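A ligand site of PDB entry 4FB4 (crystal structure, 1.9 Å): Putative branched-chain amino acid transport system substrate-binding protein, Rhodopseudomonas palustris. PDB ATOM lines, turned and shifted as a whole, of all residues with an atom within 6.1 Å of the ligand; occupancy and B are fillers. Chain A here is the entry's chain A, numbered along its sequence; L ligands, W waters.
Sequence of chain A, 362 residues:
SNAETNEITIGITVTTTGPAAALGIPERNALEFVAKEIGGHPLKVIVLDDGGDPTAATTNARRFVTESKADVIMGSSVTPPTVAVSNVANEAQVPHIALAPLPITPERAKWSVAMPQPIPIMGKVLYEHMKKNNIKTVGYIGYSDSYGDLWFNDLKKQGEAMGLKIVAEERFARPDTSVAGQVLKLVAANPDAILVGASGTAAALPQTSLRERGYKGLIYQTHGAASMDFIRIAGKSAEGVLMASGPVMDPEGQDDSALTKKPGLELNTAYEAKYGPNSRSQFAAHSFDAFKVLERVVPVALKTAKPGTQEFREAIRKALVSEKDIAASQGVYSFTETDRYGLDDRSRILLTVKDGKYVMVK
Leu 23 touches the ligand (CD2 to C5, 3.4 Å).
Ser 77 touches the ligand.
Val 78 touches the ligand (CG1 to O4, 3.5 Å).
CD of Pro 101 touches C9 of the ligand (3.4 Å).
CB of Pro 116 touches O2 of the ligand, 3.5 Å away.
Tyr 143 touches the ligand (CE2 to O4, 3.8 Å).
CD1 of Tyr 147 touches C2 of the ligand (3.4 Å).
His 223 touches the ligand.
Gly 224 touches the ligand (CA to C9, 3.5 Å).
CD1 of Phe 283 touches O3 of the ligand (3.3 Å).
Hydrophobic or aromatic side chains within 4 Å of the ligand: Leu 23, Val 78, Pro 101, Pro 116, Tyr 143, Tyr 147, His 223, Phe 283 and His 286.
Within 4 Å of the ligand: Leu 23, Ser 77, Val 78, Thr 79, Leu 99, Pro 101, Pro 116, Tyr 143, Tyr 147, Arg 174, Ser 199, His 223, Gly 224, Gln 282, Phe 283 and His 286.
The nearest printed residue that does not touch the ligand is Glu 27 (4.02 Å).
NE2 of Gln 330 is in hydrogen-bond range of OE1 of Gln 282, 2.9 Å away.
N of Tyr 147 lies within hydrogen-bond range of OD1 of Asp 145 (3.0 Å).
The side-chain hydroxyl of Tyr 147 lies within hydrogen-bond range of the side-chain hydroxyl of Thr 222 (2.6 Å).
OE1 of Gln 117 is in hydrogen-bond range of NE2 of Gln 282 (2.9 Å).
NE2 of His 223 is in hydrogen-bond range of O of Gln 117 (2.8 Å).
The guanidinium group (NE) of Arg 174 lies within salt-bridge range of the side-chain carboxylate (OD2) of Asp 145 (2.7 Å).
The side-chain hydroxyl (OG) of Ser 199 lies within hydrogen-bond range of the side-chain hydroxyl (OH) of Tyr 143.
OG of Ser 77 lies within hydrogen-bond range of OE1 of Glu 27, at 2.9 Å.
The side-chain hydroxyl of Ser 199 lies within hydrogen-bond range of an oxygen (O4) of the ligand, 2.7 Å away.
O of Leu 99 lies within hydrogen-bond range of O3 of the ligand (3.4 Å).
The side-chain amide nitrogen of Gln 282 sits at hydrogen-bond distance from an oxygen (O2) of the ligand.
O1 of the ligand lies within hydrogen-bond range of OG1 of Thr 79 (2.9 Å).
An oxygen (O1) of the ligand is in hydrogen-bond range of the backbone NH (N) of Thr 79 (2.7 Å).
The guanidinium group (NH2) of Arg 174 is in salt-bridge range of an oxygen (O4) of the ligand, 2.8 Å away.
NE2 of His 286 lies within hydrogen-bond range of O2 of the ligand (2.8 Å).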
ATOM      1  N   LEU A  23     -25.907  22.258 -24.739  1.00  0.00           N
ATOM      2  CA  LEU A  23     -26.888  21.235 -25.103  1.00  0.00           C
ATOM      3  C   LEU A  23     -28.054  21.786 -25.923  1.00  0.00           C
ATOM      4  O   LEU A  23     -28.454  21.153 -26.925  1.00  0.00           O
ATOM      5  CB  LEU A  23     -27.444  20.566 -23.849  1.00  0.00           C
ATOM      6  CG  LEU A  23     -26.464  19.585 -23.183  1.00  0.00           C
ATOM      7  CD1 LEU A  23     -25.420  20.283 -22.313  1.00  0.00           C
ATOM      8  CD2 LEU A  23     -27.233  18.587 -22.334  1.00  0.00           C
ATOM      9  N   GLU A  27     -29.750  21.409 -30.197  1.00  0.00           N
ATOM     10  CA  GLU A  27     -31.145  20.998 -30.261  1.00  0.00           C
ATOM     11  C   GLU A  27     -31.999  21.989 -31.068  1.00  0.00           C
ATOM     12  O   GLU A  27     -32.758  21.573 -31.956  1.00  0.00           O
ATOM     13  CB  GLU A  27     -31.728  20.771 -28.847  1.00  0.00           C
ATOM     14  CG  GLU A  27     -30.961  19.653 -28.165  1.00  0.00           C
ATOM     15  CD  GLU A  27     -31.226  19.440 -26.678  1.00  0.00           C
ATOM     16  OE1 GLU A  27     -31.799  20.315 -26.038  1.00  0.00           O
ATOM     17  OE2 GLU A  27     -30.846  18.342 -26.172  1.00  0.00           O
ATOM     18  N   SER A  77     -33.509  20.921 -22.010  1.00  0.00           N
ATOM     19  CA  SER A  77     -32.128  20.457 -22.331  1.00  0.00           C
ATOM     20  C   SER A  77     -31.382  19.693 -21.222  1.00  0.00           C
ATOM     21  O   SER A  77     -30.505  18.921 -21.510  1.00  0.00           O
ATOM     22  CB  SER A  77     -31.301  21.668 -22.691  1.00  0.00           C
ATOM     23  OG  SER A  77     -31.847  22.219 -23.861  1.00  0.00           O
ATOM     24  N   VAL A  78     -31.775  19.905 -20.000  1.00  0.00           N
ATOM     25  CA  VAL A  78     -31.130  19.320 -18.808  1.00  0.00           C
ATOM     26  C   VAL A  78     -32.251  18.888 -17.910  1.00  0.00           C
ATOM     27  O   VAL A  78     -33.395  19.295 -18.115  1.00  0.00           O
ATOM     28  CB  VAL A  78     -30.135  20.294 -18.112  1.00  0.00           C
ATOM     29  CG1 VAL A  78     -28.963  20.544 -19.023  1.00  0.00           C
ATOM     30  CG2 VAL A  78     -30.766  21.656 -17.733  1.00  0.00           C
ATOM     31  N   THR A  79     -31.952  18.037 -16.937  1.00  0.00           N
ATOM     32  CA  THR A  79     -32.990  17.335 -16.192  1.00  0.00           C
ATOM     33  C   THR A  79     -33.916  18.188 -15.297  1.00  0.00           C
ATOM     34  O   THR A  79     -35.122  17.969 -15.328  1.00  0.00           O
ATOM     35  CB  THR A  79     -32.341  16.223 -15.369  1.00  0.00           C
ATOM     36  OG1 THR A  79     -31.693  15.347 -16.305  1.00  0.00           O
ATOM     37  CG2 THR A  79     -33.405  15.454 -14.588  1.00  0.00           C
ATOM     38  N   PRO A  80     -33.384  19.173 -14.538  1.00  0.00           N
ATOM     39  CA  PRO A  80     -34.362  19.898 -13.623  1.00  0.00           C
ATOM     40  C   PRO A  80     -35.502  20.611 -14.325  1.00  0.00           C
ATOM     41  O   PRO A  80     -36.659  20.470 -13.881  1.00  0.00           O
ATOM     42  CB  PRO A  80     -33.476  20.849 -12.788  1.00  0.00           C
ATOM     43  CG  PRO A  80     -32.095  20.206 -12.880  1.00  0.00           C
ATOM     44  CD  PRO A  80     -31.997  19.555 -14.227  1.00  0.00           C
ATOM     45  N   LEU A  99     -36.324  16.022 -23.786  1.00  0.00           N
ATOM     46  CA  LEU A  99     -35.051  16.071 -24.453  1.00  0.00           C
ATOM     47  C   LEU A  99     -33.855  15.917 -23.510  1.00  0.00           C
ATOM     48  O   LEU A  99     -32.694  16.125 -23.914  1.00  0.00           O
ATOM     49  CB  LEU A  99     -34.938  17.363 -25.320  1.00  0.00           C
ATOM     50  CG  LEU A  99     -36.026  17.578 -26.383  1.00  0.00           C
ATOM     51  CD1 LEU A  99     -35.855  18.879 -27.188  1.00  0.00           C
ATOM     52  CD2 LEU A  99     -36.120  16.379 -27.292  1.00  0.00           C
ATOM     53  N   ALA A 100     -34.121  15.584 -22.240  1.00  0.00           N
ATOM     54  CA  ALA A 100     -33.107  15.247 -21.249  1.00  0.00           C
ATOM     55  C   ALA A 100     -33.651  14.037 -20.462  1.00  0.00           C
ATOM     56  O   ALA A 100     -34.864  13.788 -20.448  1.00  0.00           O
ATOM     57  CB  ALA A 100     -32.832  16.436 -20.303  1.00  0.00           C
ATOM     58  N   PRO A 101     -32.751  13.242 -19.868  1.00  0.00           N
ATOM     59  CA  PRO A 101     -33.247  12.133 -19.122  1.00  0.00           C
ATOM     60  C   PRO A 101     -34.010  12.696 -17.899  1.00  0.00           C
ATOM     61  O   PRO A 101     -33.760  13.822 -17.424  1.00  0.00           O
ATOM     62  CB  PRO A 101     -31.973  11.364 -18.685  1.00  0.00           C
ATOM     63  CG  PRO A 101     -30.864  11.901 -19.477  1.00  0.00           C
ATOM     64  CD  PRO A 101     -31.260  13.285 -19.890  1.00  0.00           C
ATOM     65  N   PRO A 116     -33.665  10.859 -24.765  1.00  0.00           N
ATOM     66  CA  PRO A 116     -32.295  10.406 -24.416  1.00  0.00           C
ATOM     67  C   PRO A 116     -32.307   9.011 -23.848  1.00  0.00           C
ATOM     68  O   PRO A 116     -33.295   8.583 -23.270  1.00  0.00           O
ATOM     69  CB  PRO A 116     -31.831  11.401 -23.332  1.00  0.00           C
ATOM     70  CG  PRO A 116     -32.600  12.655 -23.639  1.00  0.00           C
ATOM     71  CD  PRO A 116     -33.975  12.146 -24.120  1.00  0.00           C
ATOM     72  N   GLN A 117     -31.203   8.302 -24.036  1.00  0.00           N
ATOM     73  CA  GLN A 117     -31.069   6.943 -23.519  1.00  0.00           C
ATOM     74  C   GLN A 117     -31.241   6.908 -21.974  1.00  0.00           C
ATOM     75  O   GLN A 117     -30.712   7.763 -21.286  1.00  0.00           O
ATOM     76  CB  GLN A 117     -29.709   6.400 -23.890  1.00  0.00           C
ATOM     77  CG  GLN A 117     -29.531   6.137 -25.376  1.00  0.00           C
ATOM     78  CD  GLN A 117     -29.085   7.353 -26.148  1.00  0.00           C
ATOM     79  OE1 GLN A 117     -28.942   8.437 -25.576  1.00  0.00           O
ATOM     80  NE2 GLN A 117     -28.892   7.187 -27.464  1.00  0.00           N
ATOM     81  N   TYR A 143     -23.369  15.973 -10.134  1.00  0.00           N
ATOM     82  CA  TYR A 143     -24.192  17.066  -9.697  1.00  0.00           C
ATOM     83  C   TYR A 143     -24.959  16.737  -8.414  1.00  0.00           C
ATOM     84  O   TYR A 143     -25.409  15.597  -8.235  1.00  0.00           O
ATOM     85  CB  TYR A 143     -25.232  17.429 -10.724  1.00  0.00           C
ATOM     86  CG  TYR A 143     -24.764  17.906 -12.070  1.00  0.00           C
ATOM     87  CD1 TYR A 143     -23.628  18.704 -12.201  1.00  0.00           C
ATOM     88  CD2 TYR A 143     -25.490  17.622 -13.221  1.00  0.00           C
ATOM     89  CE1 TYR A 143     -23.233  19.168 -13.461  1.00  0.00           C
ATOM     90  CE2 TYR A 143     -25.088  18.069 -14.463  1.00  0.00           C
ATOM     91  CZ  TYR A 143     -23.959  18.878 -14.582  1.00  0.00           C
ATOM     92  OH  TYR A 143     -23.526  19.355 -15.820  1.00  0.00           O
ATOM     93  N   ASP A 145     -27.984  17.166  -7.821  1.00  0.00           N
ATOM     94  CA  ASP A 145     -29.399  17.280  -8.250  1.00  0.00           C
ATOM     95  C   ASP A 145     -29.861  15.950  -8.828  1.00  0.00           C
ATOM     96  O   ASP A 145     -29.149  14.956  -8.694  1.00  0.00           O
ATOM     97  CB  ASP A 145     -29.619  18.450  -9.228  1.00  0.00           C
ATOM     98  CG  ASP A 145     -28.926  18.254 -10.570  1.00  0.00           C
ATOM     99  OD1 ASP A 145     -28.685  17.108 -10.993  1.00  0.00           O
ATOM    100  OD2 ASP A 145     -28.619  19.307 -11.178  1.00  0.00           O
ATOM    101  N   TYR A 147     -30.173  14.634 -11.835  1.00  0.00           N
ATOM    102  CA  TYR A 147     -29.295  13.938 -12.794  1.00  0.00           C
ATOM    103  C   TYR A 147     -28.135  13.197 -12.114  1.00  0.00           C
ATOM    104  O   TYR A 147     -27.865  12.008 -12.420  1.00  0.00           O
ATOM    105  CB  TYR A 147     -28.768  14.890 -13.871  1.00  0.00           C
ATOM    106  CG  TYR A 147     -27.964  14.226 -14.941  1.00  0.00           C
ATOM    107  CD1 TYR A 147     -28.565  13.368 -15.875  1.00  0.00           C
ATOM    108  CD2 TYR A 147     -26.594  14.442 -15.043  1.00  0.00           C
ATOM    109  CE1 TYR A 147     -27.832  12.715 -16.860  1.00  0.00           C
ATOM    110  CE2 TYR A 147     -25.860  13.822 -16.044  1.00  0.00           C
ATOM    111  CZ  TYR A 147     -26.446  12.936 -16.922  1.00  0.00           C
ATOM    112  OH  TYR A 147     -25.720  12.312 -17.917  1.00  0.00           O
ATOM    113  N   ARG A 174     -24.068  22.705 -10.470  1.00  0.00           N
ATOM    114  CA  ARG A 174     -23.836  22.995 -11.875  1.00  0.00           C
ATOM    115  C   ARG A 174     -23.015  24.224 -12.114  1.00  0.00           C
ATOM    116  O   ARG A 174     -22.123  24.169 -12.961  1.00  0.00           O
ATOM    117  CB  ARG A 174     -25.157  23.124 -12.633  1.00  0.00           C
ATOM    118  CG  ARG A 174     -25.874  21.813 -12.779  1.00  0.00           C
ATOM    119  CD  ARG A 174     -27.212  21.961 -13.448  1.00  0.00           C
ATOM    120  NE  ARG A 174     -27.910  20.678 -13.367  1.00  0.00           N
ATOM    121  CZ  ARG A 174     -27.997  19.791 -14.360  1.00  0.00           C
ATOM    122  NH1 ARG A 174     -28.625  18.651 -14.152  1.00  0.00           N
ATOM    123  NH2 ARG A 174     -27.532  20.061 -15.563  1.00  0.00           N
ATOM    124  N   ALA A 198     -22.150  14.215 -14.938  1.00  0.00           N
ATOM    125  CA  ALA A 198     -22.353  15.597 -15.311  1.00  0.00           C
ATOM    126  C   ALA A 198     -22.634  15.714 -16.809  1.00  0.00           C
ATOM    127  O   ALA A 198     -22.883  14.702 -17.494  1.00  0.00           O
ATOM    128  CB  ALA A 198     -21.101  16.422 -14.943  1.00  0.00           C
ATOM    129  N   SER A 199     -22.638  16.929 -17.304  1.00  0.00           N
ATOM    130  CA  SER A 199     -23.007  17.155 -18.705  1.00  0.00           C
ATOM    131  C   SER A 199     -22.371  18.441 -19.218  1.00  0.00           C
ATOM    132  O   SER A 199     -21.961  19.304 -18.439  1.00  0.00           O
ATOM    133  CB  SER A 199     -24.497  17.212 -18.835  1.00  0.00           C
ATOM    134  OG  SER A 199     -25.038  18.305 -18.108  1.00  0.00           O
ATOM    135  N   THR A 222     -20.623  10.298 -18.823  1.00  0.00           N
ATOM    136  CA  THR A 222     -21.970   9.952 -19.251  1.00  0.00           C
ATOM    137  C   THR A 222     -22.277  10.563 -20.629  1.00  0.00           C
ATOM    138  O   THR A 222     -21.506  11.379 -21.212  1.00  0.00           O
ATOM    139  CB  THR A 222     -23.036  10.467 -18.268  1.00  0.00           C
ATOM    140  OG1 THR A 222     -23.183  11.898 -18.409  1.00  0.00           O
ATOM    141  CG2 THR A 222     -22.693  10.081 -16.847  1.00  0.00           C
ATOM    142  N   HIS A 223     -23.420  10.163 -21.148  1.00  0.00           N
ATOM    143  CA  HIS A 223     -23.885  10.642 -22.455  1.00  0.00           C
ATOM    144  C   HIS A 223     -24.237  12.120 -22.475  1.00  0.00           C
ATOM    145  O   HIS A 223     -24.348  12.713 -23.529  1.00  0.00           O
ATOM    146  CB  HIS A 223     -24.974   9.707 -23.029  1.00  0.00           C
ATOM    147  CG  HIS A 223     -26.166   9.494 -22.175  1.00  0.00           C
ATOM    148  ND1 HIS A 223     -26.098   9.264 -20.836  1.00  0.00           N
ATOM    149  CD2 HIS A 223     -27.531   9.372 -22.527  1.00  0.00           C
ATOM    150  CE1 HIS A 223     -27.351   9.040 -20.370  1.00  0.00           C
ATOM    151  NE2 HIS A 223     -28.210   9.083 -21.417  1.00  0.00           N
ATOM    152  N   GLY A 224     -24.396  12.728 -21.312  1.00  0.00           N
ATOM    153  CA  GLY A 224     -24.499  14.190 -21.229  1.00  0.00           C
ATOM    154  C   GLY A 224     -23.249  14.900 -21.685  1.00  0.00           C
ATOM    155  O   GLY A 224     -23.291  16.100 -21.948  1.00  0.00           O
ATOM    156  N   ALA A 225     -22.134  14.197 -21.806  1.00  0.00           N
ATOM    157  CA  ALA A 225     -20.879  14.839 -22.206  1.00  0.00           C
ATOM    158  C   ALA A 225     -20.574  14.689 -23.710  1.00  0.00           C
ATOM    159  O   ALA A 225     -19.585  15.196 -24.178  1.00  0.00           O
ATOM    160  CB  ALA A 225     -19.743  14.302 -21.350  1.00  0.00           C
ATOM    161  N   GLN A 282     -24.820  14.429 -29.798  1.00  0.00           N
ATOM    162  CA  GLN A 282     -25.813  13.611 -29.122  1.00  0.00           C
ATOM    163  C   GLN A 282     -27.078  14.443 -29.041  1.00  0.00           C
ATOM    164  O   GLN A 282     -28.189  13.920 -29.126  1.00  0.00           O
ATOM    165  CB  GLN A 282     -25.248  13.357 -27.708  1.00  0.00           C
ATOM    166  CG  GLN A 282     -26.177  12.810 -26.625  1.00  0.00           C
ATOM    167  CD  GLN A 282     -26.402  11.305 -26.722  1.00  0.00           C
ATOM    168  OE1 GLN A 282     -25.818  10.629 -27.570  1.00  0.00           O
ATOM    169  NE2 GLN A 282     -27.270  10.774 -25.860  1.00  0.00           N
ATOM    170  N   PHE A 283     -26.907  15.743 -28.898  1.00  0.00           N
ATOM    171  CA  PHE A 283     -28.027  16.637 -28.465  1.00  0.00           C
ATOM    172  C   PHE A 283     -28.916  17.068 -29.639  1.00  0.00           C
ATOM    173  O   PHE A 283     -30.170  16.975 -29.529  1.00  0.00           O
ATOM    174  CB  PHE A 283     -27.453  17.832 -27.696  1.00  0.00           C
ATOM    175  CG  PHE A 283     -26.443  17.431 -26.659  1.00  0.00           C
ATOM    176  CD1 PHE A 283     -26.778  16.495 -25.702  1.00  0.00           C
ATOM    177  CD2 PHE A 283     -25.161  17.923 -26.695  1.00  0.00           C
ATOM    178  CE1 PHE A 283     -25.827  16.087 -24.777  1.00  0.00           C
ATOM    179  CE2 PHE A 283     -24.220  17.532 -25.774  1.00  0.00           C
ATOM    180  CZ  PHE A 283     -24.569  16.572 -24.847  1.00  0.00           C
ATOM    181  N   HIS A 286     -31.454  14.449 -30.513  1.00  0.00           N
ATOM    182  CA  HIS A 286     -32.683  14.248 -29.733  1.00  0.00           C
ATOM    183  C   HIS A 286     -33.856  15.017 -30.279  1.00  0.00           C
ATOM    184  O   HIS A 286     -35.000  14.495 -30.320  1.00  0.00           O
ATOM    185  CB  HIS A 286     -32.494  14.576 -28.240  1.00  0.00           C
ATOM    186  CG  HIS A 286     -31.495  13.725 -27.550  1.00  0.00           C
ATOM    187  ND1 HIS A 286     -31.400  12.424 -27.747  1.00  0.00           N
ATOM    188  CD2 HIS A 286     -30.527  14.055 -26.628  1.00  0.00           C
ATOM    189  CE1 HIS A 286     -30.374  11.929 -27.025  1.00  0.00           C
ATOM    190  NE2 HIS A 286     -29.872  12.923 -26.316  1.00  0.00           N
ATOM    191  N   GLN A 330     -30.842   7.956 -32.873  1.00  0.00           N
ATOM    192  CA  GLN A 330     -30.250   7.533 -31.580  1.00  0.00           C
ATOM    193  C   GLN A 330     -30.704   6.158 -31.154  1.00  0.00           C
ATOM    194  O   GLN A 330     -30.181   5.630 -30.171  1.00  0.00           O
ATOM    195  CB  GLN A 330     -30.624   8.499 -30.470  1.00  0.00           C
ATOM    196  CG  GLN A 330     -29.945   9.857 -30.653  1.00  0.00           C
ATOM    197  CD  GLN A 330     -28.470   9.782 -30.316  1.00  0.00           C
ATOM    198  OE1 GLN A 330     -27.696   8.991 -30.914  1.00  0.00           O
ATOM    199  NE2 GLN A 330     -28.038  10.637 -29.395  1.00  0.00           N
HETATM  200  C1  LIG L   1     -28.473  16.998 -17.237  1.00  0.00           C
HETATM  201  O1  LIG L   1     -29.418  17.163 -16.451  1.00  0.00           O
HETATM  202  C2  LIG L   1     -28.417  15.872 -18.206  1.00  0.00           C
HETATM  203  C3  LIG L   1     -28.261  16.205 -19.462  1.00  0.00           C
HETATM  204  C4  LIG L   1     -28.318  15.193 -20.599  1.00  0.00           C
HETATM  205  C5  LIG L   1     -28.820  15.610 -21.816  1.00  0.00           C
HETATM  206  C6  LIG L   1     -28.937  14.752 -22.882  1.00  0.00           C
HETATM  207  C7  LIG L   1     -28.512  13.351 -22.780  1.00  0.00           C
HETATM  208  C8  LIG L   1     -28.020  12.920 -21.550  1.00  0.00           C
HETATM  209  C9  LIG L   1     -27.949  13.857 -20.484  1.00  0.00           C
HETATM  210  O2  LIG L   1     -28.623  12.549 -23.877  1.00  0.00           O
HETATM  211  O3  LIG L   1     -29.406  15.241 -24.053  1.00  0.00           O
HETATM  212  O4  LIG L   1     -27.568  17.860 -17.340  1.00  0.00           O
HETATM  213  O   HOH W   1     -30.560  17.632 -23.873  1.00  0.00           O
